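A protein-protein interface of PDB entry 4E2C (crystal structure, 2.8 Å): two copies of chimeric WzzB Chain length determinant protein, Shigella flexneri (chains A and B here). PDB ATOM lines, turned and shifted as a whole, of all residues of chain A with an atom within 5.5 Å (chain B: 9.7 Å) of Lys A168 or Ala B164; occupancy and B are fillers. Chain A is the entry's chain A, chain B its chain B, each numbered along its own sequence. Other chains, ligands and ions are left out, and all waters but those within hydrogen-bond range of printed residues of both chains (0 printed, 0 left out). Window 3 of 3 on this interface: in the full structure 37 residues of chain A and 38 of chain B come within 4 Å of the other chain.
Ala B164 touches Lys A168. Pro A169 touches Phe B183. Pro A169 touches Leu B184 (CB to CD2, 3.7 Å). Phe B183 touches Leu A185 (CZ to CB, 3.9 Å). Glu A188 touches Gln B163. Ala B164 touches Glu A188 (CA to CB, 3.8 Å). Ala A189 touches Ala B164. Phe B183 touches Ala A189 (CE1 to CB, 3.3 Å).
7 positions are printed for both chains. Of the 8 pairs that touch across the chains among the printed residues, none has its exchanged pair printed and touching as well.
Of chain B, only Ala B164 comes within 4 Å of Lys A168. Of the printed residues of chain A, Ala B164 touches Lys A168 (3.8 Å), Glu A188 (3.8 Å) and Ala A189 (3.9 Å). Pro A169 touches just these residues of chain B: Phe B183 (3.8 Å) and Leu B184 (3.7 Å). Of the printed residues of chain A, Leu B184 touches Pro A169. Of the printed residues of chain A, Gln B163 touches Glu A188 (3.8 Å). Of the printed residues of chain B, Leu A185 touches Phe B183 (3.9 Å). The nearest printed residue of chain A that does not touch Phe B183 is Gly A186 (5.8 Å).
Hydrophobic or aromatic side chains of chain B that line the printed part of chain A: Ala B164, Phe B183 and Leu B184. Printed residues of chain A that touch a printed residue of chain B: Lys A168, Pro A169, Leu A185, Glu A188 and Ala A189. Among the printed residues, no Asp or Glu carboxylate lies within 4 Å of a Lys or Arg side-chain nitrogen of the other chain.
O of Thr A167 sits close to N of Glu A188. O of Leu B184 lies within hydrogen-bond range of N of Gln B170.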
ATOM      1  N   VAL A 166      -1.792   9.368  26.588  1.00  0.00           N
ATOM      2  CA  VAL A 166      -1.089  10.540  27.104  1.00  0.00           C
ATOM      3  C   VAL A 166      -0.731  11.452  25.930  1.00  0.00           C
ATOM      4  O   VAL A 166       0.194  11.161  25.170  1.00  0.00           O
ATOM      5  CB  VAL A 166       0.188  10.144  27.865  1.00  0.00           C
ATOM      6  CG1 VAL A 166       0.941  11.375  28.296  1.00  0.00           C
ATOM      7  CG2 VAL A 166      -0.150   9.271  29.078  1.00  0.00           C
ATOM      8  N   THR A 167      -1.480  12.538  25.763  1.00  0.00           N
ATOM      9  CA  THR A 167      -1.282  13.410  24.606  1.00  0.00           C
ATOM     10  C   THR A 167      -0.360  14.594  24.902  1.00  0.00           C
ATOM     11  O   THR A 167       0.421  14.996  24.056  1.00  0.00           O
ATOM     12  CB  THR A 167      -2.613  13.987  24.104  1.00  0.00           C
ATOM     13  OG1 THR A 167      -3.054  14.988  25.027  1.00  0.00           O
ATOM     14  CG2 THR A 167      -3.643  12.913  24.015  1.00  0.00           C
ATOM     15  N   LYS A 168      -0.494  15.148  26.100  1.00  0.00           N
ATOM     16  CA  LYS A 168       0.285  16.293  26.554  1.00  0.00           C
ATOM     17  C   LYS A 168       1.309  15.809  27.574  1.00  0.00           C
ATOM     18  O   LYS A 168       1.184  14.692  28.067  1.00  0.00           O
ATOM     19  CB  LYS A 168      -0.650  17.307  27.216  1.00  0.00           C
ATOM     20  CG  LYS A 168      -1.813  17.761  26.353  1.00  0.00           C
ATOM     21  CD  LYS A 168      -1.332  18.550  25.134  1.00  0.00           C
ATOM     22  CE  LYS A 168      -2.504  19.201  24.388  1.00  0.00           C
ATOM     23  N   PRO A 169       2.315  16.644  27.905  1.00  0.00           N
ATOM     24  CA  PRO A 169       3.369  16.256  28.862  1.00  0.00           C
ATOM     25  C   PRO A 169       2.835  15.997  30.260  1.00  0.00           C
ATOM     26  O   PRO A 169       2.156  16.840  30.812  1.00  0.00           O
ATOM     27  CB  PRO A 169       4.301  17.485  28.912  1.00  0.00           C
ATOM     28  CG  PRO A 169       4.044  18.234  27.705  1.00  0.00           C
ATOM     29  CD  PRO A 169       2.601  17.937  27.266  1.00  0.00           C
ATOM     30  N   GLN A 170       3.163  14.854  30.836  1.00  0.00           N
ATOM     31  CA  GLN A 170       2.738  14.574  32.194  1.00  0.00           C
ATOM     32  C   GLN A 170       3.868  14.684  33.232  1.00  0.00           C
ATOM     33  O   GLN A 170       3.713  14.195  34.351  1.00  0.00           O
ATOM     34  CB  GLN A 170       2.078  13.193  32.276  1.00  0.00           C
ATOM     35  CG  GLN A 170       0.728  13.104  31.575  1.00  0.00           C
ATOM     36  CD  GLN A 170      -0.022  11.853  31.935  1.00  0.00           C
ATOM     37  N   LEU A 184       5.984   9.937  28.662  1.00  0.00           N
ATOM     38  CA  LEU A 184       5.472  10.966  29.546  1.00  0.00           C
ATOM     39  C   LEU A 184       5.515  12.339  28.912  1.00  0.00           C
ATOM     40  O   LEU A 184       4.856  13.245  29.385  1.00  0.00           O
ATOM     41  CB  LEU A 184       6.195  10.959  30.890  1.00  0.00           C
ATOM     42  CG  LEU A 184       5.903   9.719  31.756  1.00  0.00           C
ATOM     43  CD1 LEU A 184       6.696   9.778  33.059  1.00  0.00           C
ATOM     44  CD2 LEU A 184       4.419   9.542  32.040  1.00  0.00           C
ATOM     45  N   LEU A 185       6.257  12.499  27.827  1.00  0.00           N
ATOM     46  CA  LEU A 185       6.238  13.763  27.122  1.00  0.00           C
ATOM     47  C   LEU A 185       4.903  13.904  26.394  1.00  0.00           C
ATOM     48  O   LEU A 185       4.494  14.997  26.026  1.00  0.00           O
ATOM     49  CB  LEU A 185       7.411  13.868  26.151  1.00  0.00           C
ATOM     50  CG  LEU A 185       8.797  13.644  26.772  1.00  0.00           C
ATOM     51  CD1 LEU A 185       9.909  13.855  25.741  1.00  0.00           C
ATOM     52  CD2 LEU A 185       8.995  14.540  28.006  1.00  0.00           C
ATOM     53  N   GLY A 186       4.211  12.790  26.208  1.00  0.00           N
ATOM     54  CA  GLY A 186       2.904  12.820  25.582  1.00  0.00           C
ATOM     55  C   GLY A 186       2.996  12.691  24.083  1.00  0.00           C
ATOM     56  O   GLY A 186       4.030  12.991  23.484  1.00  0.00           O
ATOM     57  N   SER A 187       1.900  12.259  23.462  1.00  0.00           N
ATOM     58  CA  SER A 187       1.949  11.863  22.067  1.00  0.00           C
ATOM     59  C   SER A 187       2.067  13.025  21.077  1.00  0.00           C
ATOM     60  O   SER A 187       2.477  12.828  19.936  1.00  0.00           O
ATOM     61  CB  SER A 187       0.779  10.932  21.727  1.00  0.00           C
ATOM     62  OG  SER A 187      -0.447  11.624  21.819  1.00  0.00           O
ATOM     63  N   GLU A 188       1.732  14.236  21.477  1.00  0.00           N
ATOM     64  CA  GLU A 188       1.824  15.338  20.523  1.00  0.00           C
ATOM     65  C   GLU A 188       3.285  15.686  20.293  1.00  0.00           C
ATOM     66  O   GLU A 188       3.737  15.783  19.164  1.00  0.00           O
ATOM     67  CB  GLU A 188       1.046  16.569  21.015  1.00  0.00           C
ATOM     68  CG  GLU A 188      -0.310  16.267  21.601  1.00  0.00           C
ATOM     69  CD  GLU A 188      -1.443  16.866  20.812  1.00  0.00           C
ATOM     70  OE1 GLU A 188      -1.328  16.932  19.567  1.00  0.00           O
ATOM     71  OE2 GLU A 188      -2.454  17.263  21.429  1.00  0.00           O
ATOM     72  N   ALA A 189       4.004  15.896  21.386  1.00  0.00           N
ATOM     73  CA  ALA A 189       5.412  16.210  21.329  1.00  0.00           C
ATOM     74  C   ALA A 189       6.202  15.096  20.610  1.00  0.00           C
ATOM     75  O   ALA A 189       7.043  15.364  19.760  1.00  0.00           O
ATOM     76  CB  ALA A 189       5.950  16.398  22.737  1.00  0.00           C
ATOM     77  N   GLU B 156      14.689  23.290  17.342  1.00  0.00           N
ATOM     78  CA  GLU B 156      13.914  22.078  17.134  1.00  0.00           C
ATOM     79  C   GLU B 156      12.815  21.972  18.199  1.00  0.00           C
ATOM     80  O   GLU B 156      11.661  21.665  17.896  1.00  0.00           O
ATOM     81  CB  GLU B 156      14.826  20.842  17.105  1.00  0.00           C
ATOM     82  N   ALA B 157      13.181  22.256  19.444  1.00  0.00           N
ATOM     83  CA  ALA B 157      12.244  22.185  20.549  1.00  0.00           C
ATOM     84  C   ALA B 157      11.067  23.137  20.289  1.00  0.00           C
ATOM     85  O   ALA B 157       9.915  22.823  20.604  1.00  0.00           O
ATOM     86  CB  ALA B 157      12.938  22.512  21.863  1.00  0.00           C
ATOM     87  N   LEU B 158      11.352  24.290  19.702  1.00  0.00           N
ATOM     88  CA  LEU B 158      10.287  25.200  19.344  1.00  0.00           C
ATOM     89  C   LEU B 158       9.224  24.500  18.483  1.00  0.00           C
ATOM     90  O   LEU B 158       8.016  24.776  18.628  1.00  0.00           O
ATOM     91  CB  LEU B 158      10.842  26.428  18.617  1.00  0.00           C
ATOM     92  CG  LEU B 158       9.763  27.396  18.133  1.00  0.00           C
ATOM     93  CD1 LEU B 158       8.873  27.828  19.297  1.00  0.00           C
ATOM     94  CD2 LEU B 158      10.389  28.596  17.448  1.00  0.00           C
ATOM     95  N   GLN B 159       9.648  23.592  17.596  1.00  0.00           N
ATOM     96  CA  GLN B 159       8.667  22.874  16.786  1.00  0.00           C
ATOM     97  C   GLN B 159       7.810  21.898  17.613  1.00  0.00           C
ATOM     98  O   GLN B 159       6.588  21.779  17.397  1.00  0.00           O
ATOM     99  CB  GLN B 159       9.310  22.178  15.584  1.00  0.00           C
ATOM    100  CG  GLN B 159       9.903  23.134  14.563  1.00  0.00           C
ATOM    101  CD  GLN B 159      10.355  22.420  13.291  1.00  0.00           C
ATOM    102  OE1 GLN B 159      11.204  21.520  13.336  1.00  0.00           O
ATOM    103  NE2 GLN B 159       9.771  22.805  12.147  1.00  0.00           N
ATOM    104  N   TYR B 160       8.445  21.216  18.563  1.00  0.00           N
ATOM    105  CA  TYR B 160       7.722  20.296  19.416  1.00  0.00           C
ATOM    106  C   TYR B 160       6.812  21.081  20.345  1.00  0.00           C
ATOM    107  O   TYR B 160       5.702  20.654  20.641  1.00  0.00           O
ATOM    108  CB  TYR B 160       8.678  19.468  20.259  1.00  0.00           C
ATOM    109  CG  TYR B 160       9.875  18.932  19.515  1.00  0.00           C
ATOM    110  CD1 TYR B 160       9.792  18.621  18.153  1.00  0.00           C
ATOM    111  CD2 TYR B 160      11.101  18.742  20.173  1.00  0.00           C
ATOM    112  CE1 TYR B 160      10.890  18.120  17.469  1.00  0.00           C
ATOM    113  CE2 TYR B 160      12.207  18.236  19.495  1.00  0.00           C
ATOM    114  CZ  TYR B 160      12.099  17.925  18.143  1.00  0.00           C
ATOM    115  OH  TYR B 160      13.200  17.439  17.459  1.00  0.00           O
ATOM    116  N   ALA B 161       7.281  22.231  20.811  1.00  0.00           N
ATOM    117  CA  ALA B 161       6.467  23.077  21.664  1.00  0.00           C
ATOM    118  C   ALA B 161       5.232  23.563  20.903  1.00  0.00           C
ATOM    119  O   ALA B 161       4.107  23.379  21.375  1.00  0.00           O
ATOM    120  CB  ALA B 161       7.264  24.248  22.218  1.00  0.00           C
ATOM    121  N   ASN B 162       5.413  24.167  19.732  1.00  0.00           N
ATOM    122  CA  ASN B 162       4.239  24.660  19.016  1.00  0.00           C
ATOM    123  C   ASN B 162       3.220  23.540  18.840  1.00  0.00           C
ATOM    124  O   ASN B 162       2.042  23.722  19.146  1.00  0.00           O
ATOM    125  CB  ASN B 162       4.576  25.288  17.659  1.00  0.00           C
ATOM    126  CG  ASN B 162       5.341  26.591  17.795  1.00  0.00           C
ATOM    127  OD1 ASN B 162       5.160  27.314  18.768  1.00  0.00           O
ATOM    128  ND2 ASN B 162       6.229  26.881  16.832  1.00  0.00           N
ATOM    129  N   GLN B 163       3.685  22.375  18.384  1.00  0.00           N
ATOM    130  CA  GLN B 163       2.778  21.290  17.995  1.00  0.00           C
ATOM    131  C   GLN B 163       2.054  20.654  19.175  1.00  0.00           C
ATOM    132  O   GLN B 163       0.930  20.202  19.046  1.00  0.00           O
ATOM    133  CB  GLN B 163       3.531  20.232  17.195  1.00  0.00           C
ATOM    134  CG  GLN B 163       2.772  18.930  17.019  1.00  0.00           C
ATOM    135  CD  GLN B 163       3.295  18.116  15.850  1.00  0.00           C
ATOM    136  OE1 GLN B 163       4.226  18.539  15.139  1.00  0.00           O
ATOM    137  NE2 GLN B 163       2.707  16.939  15.642  1.00  0.00           N
ATOM    138  N   ALA B 164       2.720  20.611  20.322  1.00  0.00           N
ATOM    139  CA  ALA B 164       2.103  20.138  21.547  1.00  0.00           C
ATOM    140  C   ALA B 164       1.359  21.297  22.236  1.00  0.00           C
ATOM    141  O   ALA B 164       0.815  21.147  23.345  1.00  0.00           O
ATOM    142  CB  ALA B 164       3.155  19.548  22.475  1.00  0.00           C
ATOM    143  N   GLN B 165       1.365  22.459  21.582  1.00  0.00           N
ATOM    144  CA  GLN B 165       0.725  23.663  22.114  1.00  0.00           C
ATOM    145  C   GLN B 165       1.175  24.034  23.544  1.00  0.00           C
ATOM    146  O   GLN B 165       0.349  24.420  24.373  1.00  0.00           O
ATOM    147  CB  GLN B 165      -0.793  23.517  22.048  1.00  0.00           C
ATOM    148  N   VAL B 166       2.479  23.918  23.821  1.00  0.00           N
ATOM    149  CA  VAL B 166       3.053  24.323  25.105  1.00  0.00           C
ATOM    150  C   VAL B 166       3.706  25.688  24.974  1.00  0.00           C
ATOM    151  O   VAL B 166       4.843  25.798  24.484  1.00  0.00           O
ATOM    152  CB  VAL B 166       4.185  23.392  25.584  1.00  0.00           C
ATOM    153  CG1 VAL B 166       4.701  23.875  26.937  1.00  0.00           C
ATOM    154  CG2 VAL B 166       3.740  21.928  25.630  1.00  0.00           C
ATOM    155  N   THR B 167       3.014  26.724  25.438  1.00  0.00           N
ATOM    156  CA  THR B 167       3.496  28.081  25.228  1.00  0.00           C
ATOM    157  C   THR B 167       4.198  28.674  26.456  1.00  0.00           C
ATOM    158  O   THR B 167       5.049  29.534  26.327  1.00  0.00           O
ATOM    159  CB  THR B 167       2.356  29.004  24.689  1.00  0.00           C
ATOM    160  OG1 THR B 167       1.466  29.350  25.742  1.00  0.00           O
ATOM    161  CG2 THR B 167       1.557  28.287  23.612  1.00  0.00           C
ATOM    162  N   LYS B 168       3.837  28.187  27.634  1.00  0.00           N
ATOM    163  CA  LYS B 168       4.349  28.684  28.912  1.00  0.00           C
ATOM    164  C   LYS B 168       5.065  27.505  29.581  1.00  0.00           C
ATOM    165  O   LYS B 168       4.726  26.354  29.298  1.00  0.00           O
ATOM    166  CB  LYS B 168       3.172  29.155  29.775  1.00  0.00           C
ATOM    167  CG  LYS B 168       3.144  30.637  30.111  1.00  0.00           C
ATOM    168  CD  LYS B 168       2.652  31.519  28.980  1.00  0.00           C
ATOM    169  N   GLN B 170       6.371  24.385  31.638  1.00  0.00           N
ATOM    170  CA  GLN B 170       5.580  23.331  32.251  1.00  0.00           C
ATOM    171  C   GLN B 170       6.373  22.691  33.343  1.00  0.00           C
ATOM    172  O   GLN B 170       5.884  21.832  34.069  1.00  0.00           O
ATOM    173  CB  GLN B 170       5.303  22.287  31.202  1.00  0.00           C
ATOM    174  CG  GLN B 170       4.500  22.789  30.070  1.00  0.00           C
ATOM    175  CD  GLN B 170       3.175  22.133  30.041  1.00  0.00           C
ATOM    176  OE1 GLN B 170       2.987  21.068  30.630  1.00  0.00           O
ATOM    177  NE2 GLN B 170       2.227  22.759  29.362  1.00  0.00           N
ATOM    178  N   PHE B 183      11.408  21.547  25.113  1.00  0.00           N
ATOM    179  CA  PHE B 183      10.068  22.018  24.752  1.00  0.00           C
ATOM    180  C   PHE B 183       9.238  22.364  25.997  1.00  0.00           C
ATOM    181  O   PHE B 183       8.347  23.216  25.930  1.00  0.00           O
ATOM    182  CB  PHE B 183       9.321  21.073  23.762  1.00  0.00           C
ATOM    183  CG  PHE B 183       8.631  19.886  24.414  1.00  0.00           C
ATOM    184  CD1 PHE B 183       7.253  19.781  24.408  1.00  0.00           C
ATOM    185  CD2 PHE B 183       9.363  18.866  24.997  1.00  0.00           C
ATOM    186  CE1 PHE B 183       6.612  18.686  24.996  1.00  0.00           C
ATOM    187  CE2 PHE B 183       8.734  17.771  25.583  1.00  0.00           C
ATOM    188  CZ  PHE B 183       7.364  17.677  25.583  1.00  0.00           C
ATOM    189  N   LEU B 184       9.557  21.736  27.127  1.00  0.00           N
ATOM    190  CA  LEU B 184       8.851  22.022  28.375  1.00  0.00           C
ATOM    191  C   LEU B 184       9.011  23.477  28.828  1.00  0.00           C
ATOM    192  O   LEU B 184       8.189  23.997  29.588  1.00  0.00           O
ATOM    193  CB  LEU B 184       9.270  21.060  29.478  1.00  0.00           C
ATOM    194  CG  LEU B 184       8.969  19.609  29.102  1.00  0.00           C
ATOM    195  CD1 LEU B 184       9.605  18.631  30.093  1.00  0.00           C
ATOM    196  CD2 LEU B 184       7.475  19.373  28.981  1.00  0.00           C
ATOM    197  N   GLY B 186       8.435  25.796  26.895  1.00  0.00           N
ATOM    198  CA  GLY B 186       7.345  26.482  26.215  1.00  0.00           C
ATOM    199  C   GLY B 186       7.755  27.423  25.093  1.00  0.00           C
ATOM    200  O   GLY B 186       8.789  28.095  25.154  1.00  0.00           O
ATOM    201  N   SER B 187       6.921  27.484  24.062  1.00  0.00           N
ATOM    202  CA  SER B 187       7.249  28.220  22.845  1.00  0.00           C
ATOM    203  C   SER B 187       7.621  29.689  23.072  1.00  0.00           C
ATOM    204  O   SER B 187       8.429  30.254  22.341  1.00  0.00           O
ATOM    205  CB  SER B 187       6.106  28.102  21.822  1.00  0.00           C
ATOM    206  OG  SER B 187       4.920  28.769  22.255  1.00  0.00           O
